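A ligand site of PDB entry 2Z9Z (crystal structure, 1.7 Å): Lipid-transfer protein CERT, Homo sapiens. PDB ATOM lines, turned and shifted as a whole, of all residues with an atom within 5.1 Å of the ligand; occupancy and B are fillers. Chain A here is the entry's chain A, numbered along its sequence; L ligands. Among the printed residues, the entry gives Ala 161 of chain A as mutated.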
ATOM      1  N   PHE A  93     -14.181 -26.725   0.907  1.00  0.00           N
ATOM      2  CA  PHE A  93     -14.956 -25.512   1.176  1.00  0.00           C
ATOM      3  C   PHE A  93     -16.287 -25.851   1.842  1.00  0.00           C
ATOM      4  O   PHE A  93     -16.730 -25.118   2.735  1.00  0.00           O
ATOM      5  CB  PHE A  93     -15.200 -24.761  -0.127  1.00  0.00           C
ATOM      6  CG  PHE A  93     -15.821 -23.381   0.031  1.00  0.00           C
ATOM      7  CD1 PHE A  93     -15.126 -22.316   0.603  1.00  0.00           C
ATOM      8  CD2 PHE A  93     -17.110 -23.140  -0.445  1.00  0.00           C
ATOM      9  CE1 PHE A  93     -15.727 -21.032   0.728  1.00  0.00           C
ATOM     10  CE2 PHE A  93     -17.719 -21.869  -0.330  1.00  0.00           C
ATOM     11  CZ  PHE A  93     -17.020 -20.824   0.262  1.00  0.00           C
ATOM     12  N   TRP A  94     -16.895 -26.964   1.421  1.00  0.00           N
ATOM     13  CA  TRP A  94     -18.221 -27.400   1.894  1.00  0.00           C
ATOM     14  C   TRP A  94     -18.197 -28.225   3.179  1.00  0.00           C
ATOM     15  O   TRP A  94     -19.145 -28.154   3.988  1.00  0.00           O
ATOM     16  CB  TRP A  94     -18.893 -28.243   0.809  1.00  0.00           C
ATOM     17  CG  TRP A  94     -20.297 -28.669   1.130  1.00  0.00           C
ATOM     18  CD1 TRP A  94     -21.443 -27.929   0.984  1.00  0.00           C
ATOM     19  CD2 TRP A  94     -20.709 -29.941   1.639  1.00  0.00           C
ATOM     20  NE1 TRP A  94     -22.542 -28.663   1.363  1.00  0.00           N
ATOM     21  CE2 TRP A  94     -22.119 -29.904   1.764  1.00  0.00           C
ATOM     22  CE3 TRP A  94     -20.025 -31.108   2.000  1.00  0.00           C
ATOM     23  CZ2 TRP A  94     -22.853 -30.995   2.242  1.00  0.00           C
ATOM     24  CZ3 TRP A  94     -20.750 -32.186   2.457  1.00  0.00           C
ATOM     25  CH2 TRP A  94     -22.154 -32.128   2.584  1.00  0.00           C
ATOM     26  N   ARG A  99     -13.904 -26.934   8.554  1.00  0.00           N
ATOM     27  CA  ARG A  99     -14.061 -25.456   8.597  1.00  0.00           C
ATOM     28  C   ARG A  99     -13.095 -24.733   9.535  1.00  0.00           C
ATOM     29  O   ARG A  99     -12.575 -23.669   9.212  1.00  0.00           O
ATOM     30  CB  ARG A  99     -15.493 -25.053   8.993  1.00  0.00           C
ATOM     31  CG  ARG A  99     -16.603 -25.468   8.021  1.00  0.00           C
ATOM     32  CD  ARG A  99     -16.846 -24.446   6.897  1.00  0.00           C
ATOM     33  NE  ARG A  99     -17.766 -24.984   5.875  1.00  0.00           N
ATOM     34  CZ  ARG A  99     -19.065 -24.705   5.811  1.00  0.00           C
ATOM     35  NH1 ARG A  99     -19.619 -23.871   6.684  1.00  0.00           N
ATOM     36  NH2 ARG A  99     -19.822 -25.252   4.853  1.00  0.00           N
ATOM     37  N   TRP A 102      -9.299 -23.698   8.474  1.00  0.00           N
ATOM     38  CA  TRP A 102      -9.009 -22.613   7.515  1.00  0.00           C
ATOM     39  C   TRP A 102      -9.762 -21.303   7.778  1.00  0.00           C
ATOM     40  O   TRP A 102      -9.238 -20.220   7.515  1.00  0.00           O
ATOM     41  CB  TRP A 102      -9.190 -23.101   6.064  1.00  0.00           C
ATOM     42  CG  TRP A 102     -10.573 -23.577   5.723  1.00  0.00           C
ATOM     43  CD1 TRP A 102     -11.040 -24.858   5.760  1.00  0.00           C
ATOM     44  CD2 TRP A 102     -11.675 -22.759   5.291  1.00  0.00           C
ATOM     45  NE1 TRP A 102     -12.368 -24.893   5.385  1.00  0.00           N
ATOM     46  CE2 TRP A 102     -12.780 -23.621   5.085  1.00  0.00           C
ATOM     47  CE3 TRP A 102     -11.833 -21.387   5.060  1.00  0.00           C
ATOM     48  CZ2 TRP A 102     -14.025 -23.149   4.658  1.00  0.00           C
ATOM     49  CZ3 TRP A 102     -13.079 -20.914   4.643  1.00  0.00           C
ATOM     50  CH2 TRP A 102     -14.158 -21.802   4.437  1.00  0.00           C
ATOM     51  N   GLU A 103     -10.991 -21.413   8.283  1.00  0.00           N
ATOM     52  CA  GLU A 103     -11.839 -20.234   8.499  1.00  0.00           C
ATOM     53  C   GLU A 103     -11.474 -19.521   9.802  1.00  0.00           C
ATOM     54  O   GLU A 103     -11.295 -20.165  10.837  1.00  0.00           O
ATOM     55  CB  GLU A 103     -13.321 -20.627   8.489  1.00  0.00           C
ATOM     56  CG  GLU A 103     -14.272 -19.549   9.050  1.00  0.00           C
ATOM     57  CD  GLU A 103     -14.260 -18.269   8.230  1.00  0.00           C
ATOM     58  OE1 GLU A 103     -14.267 -18.339   6.976  1.00  0.00           O
ATOM     59  OE2 GLU A 103     -14.245 -17.180   8.825  1.00  0.00           O
ATOM     60  N   THR A 105     -12.994 -15.984  10.667  1.00  0.00           N
ATOM     61  CA  THR A 105     -14.079 -15.084  11.118  1.00  0.00           C
ATOM     62  C   THR A 105     -15.273 -15.754  11.837  1.00  0.00           C
ATOM     63  O   THR A 105     -16.096 -15.059  12.419  1.00  0.00           O
ATOM     64  CB  THR A 105     -14.611 -14.191   9.952  1.00  0.00           C
ATOM     65  OG1 THR A 105     -15.514 -14.945   9.124  1.00  0.00           O
ATOM     66  CG2 THR A 105     -13.492 -13.685   9.096  1.00  0.00           C
ATOM     67  N   ILE A 106     -15.371 -17.079  11.792  1.00  0.00           N
ATOM     68  CA  ILE A 106     -16.494 -17.784  12.432  1.00  0.00           C
ATOM     69  C   ILE A 106     -16.209 -18.112  13.900  1.00  0.00           C
ATOM     70  O   ILE A 106     -15.135 -18.627  14.231  1.00  0.00           O
ATOM     71  CB  ILE A 106     -16.901 -19.082  11.670  1.00  0.00           C
ATOM     72  CG1 ILE A 106     -17.486 -18.746  10.294  1.00  0.00           C
ATOM     73  CG2 ILE A 106     -17.890 -19.917  12.479  1.00  0.00           C
ATOM     74  CD1 ILE A 106     -17.695 -19.938   9.380  1.00  0.00           C
ATOM     75  N   GLN A 124     -24.709 -20.200  12.036  1.00  0.00           N
ATOM     76  CA  GLN A 124     -23.405 -19.765  12.543  1.00  0.00           C
ATOM     77  C   GLN A 124     -23.378 -18.312  13.020  1.00  0.00           C
ATOM     78  O   GLN A 124     -24.119 -17.450  12.538  1.00  0.00           O
ATOM     79  CB  GLN A 124     -22.283 -19.999  11.513  1.00  0.00           C
ATOM     80  CG  GLN A 124     -22.317 -19.085  10.290  1.00  0.00           C
ATOM     81  CD  GLN A 124     -21.312 -19.496   9.232  1.00  0.00           C
ATOM     82  OE1 GLN A 124     -21.007 -20.675   9.082  1.00  0.00           O
ATOM     83  NE2 GLN A 124     -20.818 -18.538   8.475  1.00  0.00           N
ATOM     84  N   HIS A 126     -20.533 -15.050  13.847  1.00  0.00           N
ATOM     85  CA  HIS A 126     -19.240 -14.561  13.405  1.00  0.00           C
ATOM     86  C   HIS A 126     -18.593 -13.744  14.489  1.00  0.00           C
ATOM     87  O   HIS A 126     -19.261 -13.032  15.245  1.00  0.00           O
ATOM     88  CB  HIS A 126     -19.389 -13.680  12.158  1.00  0.00           C
ATOM     89  CG  HIS A 126     -19.631 -14.452  10.907  1.00  0.00           C
ATOM     90  ND1 HIS A 126     -18.602 -14.812  10.061  1.00  0.00           N
ATOM     91  CD2 HIS A 126     -20.770 -14.944  10.362  1.00  0.00           C
ATOM     92  CE1 HIS A 126     -19.104 -15.499   9.035  1.00  0.00           C
ATOM     93  NE2 HIS A 126     -20.419 -15.587   9.199  1.00  0.00           N
ATOM     94  N   VAL A 129     -15.810  -8.438  13.247  1.00  0.00           N
ATOM     95  CA  VAL A 129     -14.798  -7.942  12.288  1.00  0.00           C
ATOM     96  C   VAL A 129     -14.796  -6.416  12.146  1.00  0.00           C
ATOM     97  O   VAL A 129     -13.860  -5.853  11.558  1.00  0.00           O
ATOM     98  CB  VAL A 129     -14.879  -8.636  10.913  1.00  0.00           C
ATOM     99  CG1 VAL A 129     -14.226 -10.006  10.986  1.00  0.00           C
ATOM    100  CG2 VAL A 129     -16.312  -8.741  10.422  1.00  0.00           C
ATOM    101  N   TRP A 130     -15.831  -5.773  12.661  1.00  0.00           N
ATOM    102  CA  TRP A 130     -15.773  -4.340  12.948  1.00  0.00           C
ATOM    103  C   TRP A 130     -16.402  -4.127  14.340  1.00  0.00           C
ATOM    104  O   TRP A 130     -17.173  -4.980  14.794  1.00  0.00           O
ATOM    105  CB  TRP A 130     -16.445  -3.518  11.836  1.00  0.00           C
ATOM    106  CG  TRP A 130     -17.923  -3.713  11.702  1.00  0.00           C
ATOM    107  CD1 TRP A 130     -18.902  -3.010  12.340  1.00  0.00           C
ATOM    108  CD2 TRP A 130     -18.591  -4.664  10.864  1.00  0.00           C
ATOM    109  NE1 TRP A 130     -20.145  -3.468  11.974  1.00  0.00           N
ATOM    110  CE2 TRP A 130     -19.980  -4.492  11.065  1.00  0.00           C
ATOM    111  CE3 TRP A 130     -18.156  -5.664   9.973  1.00  0.00           C
ATOM    112  CZ2 TRP A 130     -20.946  -5.263  10.395  1.00  0.00           C
ATOM    113  CZ3 TRP A 130     -19.122  -6.435   9.313  1.00  0.00           C
ATOM    114  CH2 TRP A 130     -20.496  -6.241   9.535  1.00  0.00           C
ATOM    115  N   ARG A 135     -22.573 -10.754  14.042  1.00  0.00           N
ATOM    116  CA  ARG A 135     -23.537 -11.179  13.033  1.00  0.00           C
ATOM    117  C   ARG A 135     -23.752 -12.655  13.161  1.00  0.00           C
ATOM    118  O   ARG A 135     -22.824 -13.403  13.461  1.00  0.00           O
ATOM    119  CB  ARG A 135     -23.039 -10.846  11.615  1.00  0.00           C
ATOM    120  CG  ARG A 135     -23.635  -9.573  11.020  1.00  0.00           C
ATOM    121  CD  ARG A 135     -23.266  -8.345  11.819  1.00  0.00           C
ATOM    122  NE  ARG A 135     -24.006  -7.187  11.347  1.00  0.00           N
ATOM    123  CZ  ARG A 135     -24.032  -5.993  11.954  1.00  0.00           C
ATOM    124  NH1 ARG A 135     -23.362  -5.806  13.088  1.00  0.00           N
ATOM    125  NH2 ARG A 135     -24.755  -5.014  11.437  1.00  0.00           N
ATOM    126  N   VAL A 137     -25.781 -15.976  10.821  1.00  0.00           N
ATOM    127  CA  VAL A 137     -26.209 -16.323   9.468  1.00  0.00           C
ATOM    128  C   VAL A 137     -26.886 -17.677   9.518  1.00  0.00           C
ATOM    129  O   VAL A 137     -26.502 -18.539  10.311  1.00  0.00           O
ATOM    130  CB  VAL A 137     -25.006 -16.409   8.466  1.00  0.00           C
ATOM    131  CG1 VAL A 137     -25.509 -16.218   7.028  1.00  0.00           C
ATOM    132  CG2 VAL A 137     -23.922 -15.360   8.787  1.00  0.00           C
ATOM    133  N   TYR A 139     -28.070 -20.381   6.540  1.00  0.00           N
ATOM    134  CA  TYR A 139     -27.984 -20.580   5.114  1.00  0.00           C
ATOM    135  C   TYR A 139     -27.970 -22.047   4.728  1.00  0.00           C
ATOM    136  O   TYR A 139     -27.527 -22.897   5.513  1.00  0.00           O
ATOM    137  CB  TYR A 139     -26.729 -19.881   4.538  1.00  0.00           C
ATOM    138  CG  TYR A 139     -25.403 -20.371   5.107  1.00  0.00           C
ATOM    139  CD1 TYR A 139     -24.628 -21.318   4.426  1.00  0.00           C
ATOM    140  CD2 TYR A 139     -24.919 -19.876   6.316  1.00  0.00           C
ATOM    141  CE1 TYR A 139     -23.402 -21.757   4.953  1.00  0.00           C
ATOM    142  CE2 TYR A 139     -23.705 -20.307   6.853  1.00  0.00           C
ATOM    143  CZ  TYR A 139     -22.951 -21.248   6.152  1.00  0.00           C
ATOM    144  OH  TYR A 139     -21.757 -21.683   6.679  1.00  0.00           O
ATOM    145  N   SER A 141     -26.239 -24.737   2.414  1.00  0.00           N
ATOM    146  CA  SER A 141     -24.920 -24.901   1.782  1.00  0.00           C
ATOM    147  C   SER A 141     -24.988 -26.212   1.048  1.00  0.00           C
ATOM    148  O   SER A 141     -25.275 -27.256   1.638  1.00  0.00           O
ATOM    149  CB  SER A 141     -23.819 -24.960   2.839  1.00  0.00           C
ATOM    150  OG  SER A 141     -22.541 -25.175   2.244  1.00  0.00           O
ATOM    151  N   VAL A 159     -20.111 -24.767  -4.857  1.00  0.00           N
ATOM    152  CA  VAL A 159     -20.709 -24.791  -3.541  1.00  0.00           C
ATOM    153  C   VAL A 159     -21.460 -23.465  -3.458  1.00  0.00           C
ATOM    154  O   VAL A 159     -20.864 -22.400  -3.629  1.00  0.00           O
ATOM    155  CB  VAL A 159     -19.669 -24.864  -2.416  1.00  0.00           C
ATOM    156  CG1 VAL A 159     -20.333 -24.821  -1.061  1.00  0.00           C
ATOM    157  CG2 VAL A 159     -18.793 -26.143  -2.535  1.00  0.00           C
ATOM    158  N   ALA A 161     -23.959 -21.088  -1.044  1.00  0.00           N
ATOM    159  CA  ALA A 161     -24.342 -20.825   0.335  1.00  0.00           C
ATOM    160  C   ALA A 161     -25.277 -19.625   0.280  1.00  0.00           C
ATOM    161  O   ALA A 161     -24.880 -18.542  -0.166  1.00  0.00           O
ATOM    162  CB  ALA A 161     -23.144 -20.522   1.186  1.00  0.00           C
ATOM    163  N   ALA A 178     -27.272 -11.451   9.286  1.00  0.00           N
ATOM    164  CA  ALA A 178     -26.766 -11.169   7.947  1.00  0.00           C
ATOM    165  C   ALA A 178     -27.497 -12.037   6.960  1.00  0.00           C
ATOM    166  O   ALA A 178     -27.980 -13.135   7.303  1.00  0.00           O
ATOM    167  CB  ALA A 178     -25.250 -11.431   7.867  1.00  0.00           C
ATOM    168  N   ILE A 180     -26.897 -13.742   3.118  1.00  0.00           N
ATOM    169  CA  ILE A 180     -25.814 -14.048   2.175  1.00  0.00           C
ATOM    170  C   ILE A 180     -26.241 -14.765   0.910  1.00  0.00           C
ATOM    171  O   ILE A 180     -27.229 -15.526   0.871  1.00  0.00           O
ATOM    172  CB  ILE A 180     -24.662 -14.852   2.849  1.00  0.00           C
ATOM    173  CG1 ILE A 180     -25.134 -16.266   3.252  1.00  0.00           C
ATOM    174  CG2 ILE A 180     -24.091 -14.073   3.999  1.00  0.00           C
ATOM    175  CD1 ILE A 180     -24.008 -17.305   3.338  1.00  0.00           C
ATOM    176  N   VAL A 182     -23.481 -16.606  -1.610  1.00  0.00           N
ATOM    177  CA  VAL A 182     -22.031 -16.827  -1.801  1.00  0.00           C
ATOM    178  C   VAL A 182     -21.884 -18.070  -2.667  1.00  0.00           C
ATOM    179  O   VAL A 182     -22.664 -19.029  -2.537  1.00  0.00           O
ATOM    180  CB  VAL A 182     -21.322 -17.067  -0.419  1.00  0.00           C
ATOM    181  CG1 VAL A 182     -19.914 -17.643  -0.602  1.00  0.00           C
ATOM    182  CG2 VAL A 182     -21.232 -15.785   0.435  1.00  0.00           C
ATOM    183  N   TYR A 210     -15.046 -16.920  -7.060  1.00  0.00           N
ATOM    184  CA  TYR A 210     -15.719 -16.825  -5.773  1.00  0.00           C
ATOM    185  C   TYR A 210     -16.560 -15.536  -5.813  1.00  0.00           C
ATOM    186  O   TYR A 210     -16.048 -14.483  -6.167  1.00  0.00           O
ATOM    187  CB  TYR A 210     -14.688 -16.748  -4.643  1.00  0.00           C
ATOM    188  CG  TYR A 210     -15.294 -16.437  -3.298  1.00  0.00           C
ATOM    189  CD1 TYR A 210     -15.839 -17.447  -2.523  1.00  0.00           C
ATOM    190  CD2 TYR A 210     -15.310 -15.127  -2.796  1.00  0.00           C
ATOM    191  CE1 TYR A 210     -16.387 -17.203  -1.308  1.00  0.00           C
ATOM    192  CE2 TYR A 210     -15.872 -14.866  -1.561  1.00  0.00           C
ATOM    193  CZ  TYR A 210     -16.422 -15.895  -0.827  1.00  0.00           C
ATOM    194  OH  TYR A 210     -16.992 -15.697   0.406  1.00  0.00           O
ATOM    195  N   VAL A 214     -23.463  -9.963   0.143  1.00  0.00           N
ATOM    196  CA  VAL A 214     -23.770 -10.032   1.554  1.00  0.00           C
ATOM    197  C   VAL A 214     -24.483  -8.749   1.977  1.00  0.00           C
ATOM    198  O   VAL A 214     -24.071  -7.644   1.582  1.00  0.00           O
ATOM    199  CB  VAL A 214     -22.483 -10.273   2.400  1.00  0.00           C
ATOM    200  CG1 VAL A 214     -22.778 -10.159   3.907  1.00  0.00           C
ATOM    201  CG2 VAL A 214     -21.858 -11.637   2.042  1.00  0.00           C
ATOM    202  N   VAL A 228     -13.327  -3.537   5.730  1.00  0.00           N
ATOM    203  CA  VAL A 228     -13.421  -4.918   6.244  1.00  0.00           C
ATOM    204  C   VAL A 228     -13.457  -5.914   5.060  1.00  0.00           C
ATOM    205  O   VAL A 228     -12.671  -6.867   5.040  1.00  0.00           O
ATOM    206  CB  VAL A 228     -14.618  -5.156   7.207  1.00  0.00           C
ATOM    207  CG1 VAL A 228     -14.710  -6.625   7.588  1.00  0.00           C
ATOM    208  CG2 VAL A 228     -14.494  -4.308   8.488  1.00  0.00           C
ATOM    209  N   ALA A 229     -14.317  -5.645   4.076  1.00  0.00           N
ATOM    210  CA  ALA A 229     -14.436  -6.484   2.886  1.00  0.00           C
ATOM    211  C   ALA A 229     -13.085  -6.640   2.174  1.00  0.00           C
ATOM    212  O   ALA A 229     -12.655  -7.760   1.890  1.00  0.00           O
ATOM    213  CB  ALA A 229     -15.470  -5.914   1.927  1.00  0.00           C
ATOM    214  N   GLU A 232     -10.835  -8.899   4.542  1.00  0.00           N
ATOM    215  CA  GLU A 232     -11.240 -10.238   4.939  1.00  0.00           C
ATOM    216  C   GLU A 232     -11.349 -11.229   3.784  1.00  0.00           C
ATOM    217  O   GLU A 232     -10.967 -12.381   3.927  1.00  0.00           O
ATOM    218  CB  GLU A 232     -12.528 -10.205   5.768  1.00  0.00           C
ATOM    219  CG  GLU A 232     -12.359  -9.709   7.220  1.00  0.00           C
ATOM    220  CD  GLU A 232     -11.205 -10.383   7.968  1.00  0.00           C
ATOM    221  OE1 GLU A 232     -11.128 -11.623   7.991  1.00  0.00           O
ATOM    222  OE2 GLU A 232     -10.359  -9.665   8.553  1.00  0.00           O
ATOM    223  N   TYR A 233     -11.821 -10.784   2.615  1.00  0.00           N
ATOM    224  CA  TYR A 233     -11.974 -11.714   1.481  1.00  0.00           C
ATOM    225  C   TYR A 233     -10.642 -12.244   0.877  1.00  0.00           C
ATOM    226  O   TYR A 233     -10.480 -13.472   0.722  1.00  0.00           O
ATOM    227  CB  TYR A 233     -12.907 -11.171   0.404  1.00  0.00           C
ATOM    228  CG  TYR A 233     -14.365 -11.141   0.818  1.00  0.00           C
ATOM    229  CD1 TYR A 233     -14.957  -9.946   1.231  1.00  0.00           C
ATOM    230  CD2 TYR A 233     -15.141 -12.300   0.821  1.00  0.00           C
ATOM    231  CE1 TYR A 233     -16.288  -9.890   1.619  1.00  0.00           C
ATOM    232  CE2 TYR A 233     -16.487 -12.267   1.208  1.00  0.00           C
ATOM    233  CZ  TYR A 233     -17.054 -11.046   1.603  1.00  0.00           C
ATOM    234  OH  TYR A 233     -18.384 -10.990   1.981  1.00  0.00           O
ATOM    235  N   PHE A 236      -9.060 -14.665   3.453  1.00  0.00           N
ATOM    236  CA  PHE A 236      -9.748 -15.947   3.405  1.00  0.00           C
ATOM    237  C   PHE A 236      -9.301 -16.752   2.179  1.00  0.00           C
ATOM    238  O   PHE A 236      -8.945 -17.929   2.331  1.00  0.00           O
ATOM    239  CB  PHE A 236     -11.272 -15.737   3.433  1.00  0.00           C
ATOM    240  CG  PHE A 236     -12.013 -16.669   2.503  1.00  0.00           C
ATOM    241  CD1 PHE A 236     -11.996 -18.050   2.730  1.00  0.00           C
ATOM    242  CD2 PHE A 236     -12.672 -16.161   1.392  1.00  0.00           C
ATOM    243  CE1 PHE A 236     -12.660 -18.918   1.865  1.00  0.00           C
ATOM    244  CE2 PHE A 236     -13.329 -17.017   0.517  1.00  0.00           C
ATOM    245  CZ  PHE A 236     -13.312 -18.398   0.754  1.00  0.00           C
HETATM  246  O1  LIG L   1     -19.202 -19.137   6.105  1.00  0.00           O
HETATM  247  C1  LIG L   1     -19.791 -19.289   5.034  1.00  0.00           C
HETATM  248  C2  LIG L   1     -20.489 -18.107   4.393  1.00  0.00           C
HETATM  249  C3  LIG L   1     -19.826 -16.821   4.861  1.00  0.00           C
HETATM  250  C4  LIG L   1     -20.395 -15.611   4.145  1.00  0.00           C
HETATM  251  C5  LIG L   1     -19.829 -14.305   4.671  1.00  0.00           C
HETATM  252  C6  LIG L   1     -20.693 -13.746   5.798  1.00  0.00           C
HETATM  253  C7  LIG L   1     -20.429 -12.258   6.002  1.00  0.00           C
HETATM  254  C8  LIG L   1     -21.357 -11.679   7.068  1.00  0.00           C
HETATM  255  C9  LIG L   1     -20.608 -11.449   8.375  1.00  0.00           C
HETATM  256  C10 LIG L   1     -20.590  -9.985   8.752  1.00  0.00           C
HETATM  257  O2  LIG L   1     -19.791 -20.599   4.392  1.00  0.00           O
HETATM  258  C11 LIG L   1     -18.467 -21.099   4.139  1.00  0.00           C
HETATM  259  C12 LIG L   1     -18.422 -22.470   3.456  1.00  0.00           C
HETATM  260  O3  LIG L   1     -19.740 -22.975   3.167  1.00  0.00           O
HETATM  261  C13 LIG L   1     -17.793 -20.140   3.176  1.00  0.00           C
HETATM  262  O4  LIG L   1     -17.069 -19.133   3.857  1.00  0.00           O
HETATM  263  C14 LIG L   1     -16.687 -17.972   3.073  1.00  0.00           C
HETATM  264  O5  LIG L   1     -17.385 -17.701   2.103  1.00  0.00           O
HETATM  265  C15 LIG L   1     -15.457 -17.149   3.421  1.00  0.00           C
HETATM  266  C16 LIG L   1     -15.595 -16.313   4.695  1.00  0.00           C
HETATM  267  C17 LIG L   1     -14.971 -14.937   4.555  1.00  0.00           C
HETATM  268  C18 LIG L   1     -16.014 -13.872   4.892  1.00  0.00           C
HETATM  269  C19 LIG L   1     -15.503 -12.448   4.770  1.00  0.00           C
HETATM  270  C20 LIG L   1     -16.192 -11.574   5.801  1.00  0.00           C
HETATM  271  C21 LIG L   1     -17.142 -10.566   5.159  1.00  0.00           C
HETATM  272  C22 LIG L   1     -16.869  -9.178   5.700  1.00  0.00           C
HETATM  273  C23 LIG L   1     -18.097  -8.292   5.617  1.00  0.00           C
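OH of Tyr 139 lies within hydrogen-bond range of OE1 of Gln 124 (2.7 Å).
NE2 of Gln 124 sits at hydrogen-bond distance from NE2 of His 126 (3.1 Å).
N of Val 137 sits at hydrogen-bond distance from O of Gln 124 (2.8 Å).
The side-chain carboxylate (OE2) of Glu 103 sits at hydrogen-bond distance from the backbone NH (N) of Ile 106, 3.2 Å away.
The side-chain carboxylate (OE2) of Glu 103 lies within hydrogen-bond range of the backbone NH (N) of Thr 105, 2.5 Å away.
NE1 of Trp 94 lies within hydrogen-bond range of O of Ser 141, at 3.1 Å.
The backbone carbonyl oxygen (O) of Ala 161 sits at hydrogen-bond distance from the backbone NH (N) of Val 182, 2.8 Å away.
The backbone NH (N) of His 126 is in hydrogen-bond range of the backbone carbonyl oxygen (O) of Arg 135.
Phe 93 touches the ligand.
Trp 102 touches the ligand.
OE1 of Glu 103 touches C16 of the ligand, at 3.3 Å.
Ile 106 touches the ligand (CD1 to O1, 3.7 Å).
NE2 of His 126 touches C6 of the ligand, 3.9 Å away.
Trp 130 touches the ligand.
Arg 135 touches the ligand (CG to C10, 3.8 Å).
Ser 141 touches the ligand.
CB of Ala 178 touches C8 of the ligand (3.98 Å).
Ile 180 touches the ligand.
Val 182 touches the ligand.
Val 214 touches the ligand.
Val 228 touches the ligand.
Glu 232 touches the ligand (CB to C19, 3.9 Å).
OH of Tyr 233 touches C21 of the ligand (3.4 Å).
Phe 236 touches the ligand (CD2 to C15, 3.6 Å).
Hydrophobic or aromatic side chains within 4 Å of the ligand: Phe 93, Trp 102, Ile 106, Trp 130, Tyr 139, Ala 178, Ile 180, Val 182, Tyr 210, Val 214, Val 228, Tyr 233 and Phe 236.
Along chain A the residues within 4 Å of the ligand span positions 93 to 236.
An oxygen (O5) of the ligand sits at hydrogen-bond distance from the side-chain hydroxyl (OH) of Tyr 210, 2.7 Å away.
The guanidinium group (NH2) of Arg 99 sits at hydrogen-bond distance from an oxygen (O3) of the ligand, 2.8 Å away.
NE2 of Gln 124 sits at hydrogen-bond distance from O1 of the ligand, at 2.9 Å.
OH of Tyr 139 sits at hydrogen-bond distance from O2 of the ligand (3.2 Å).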
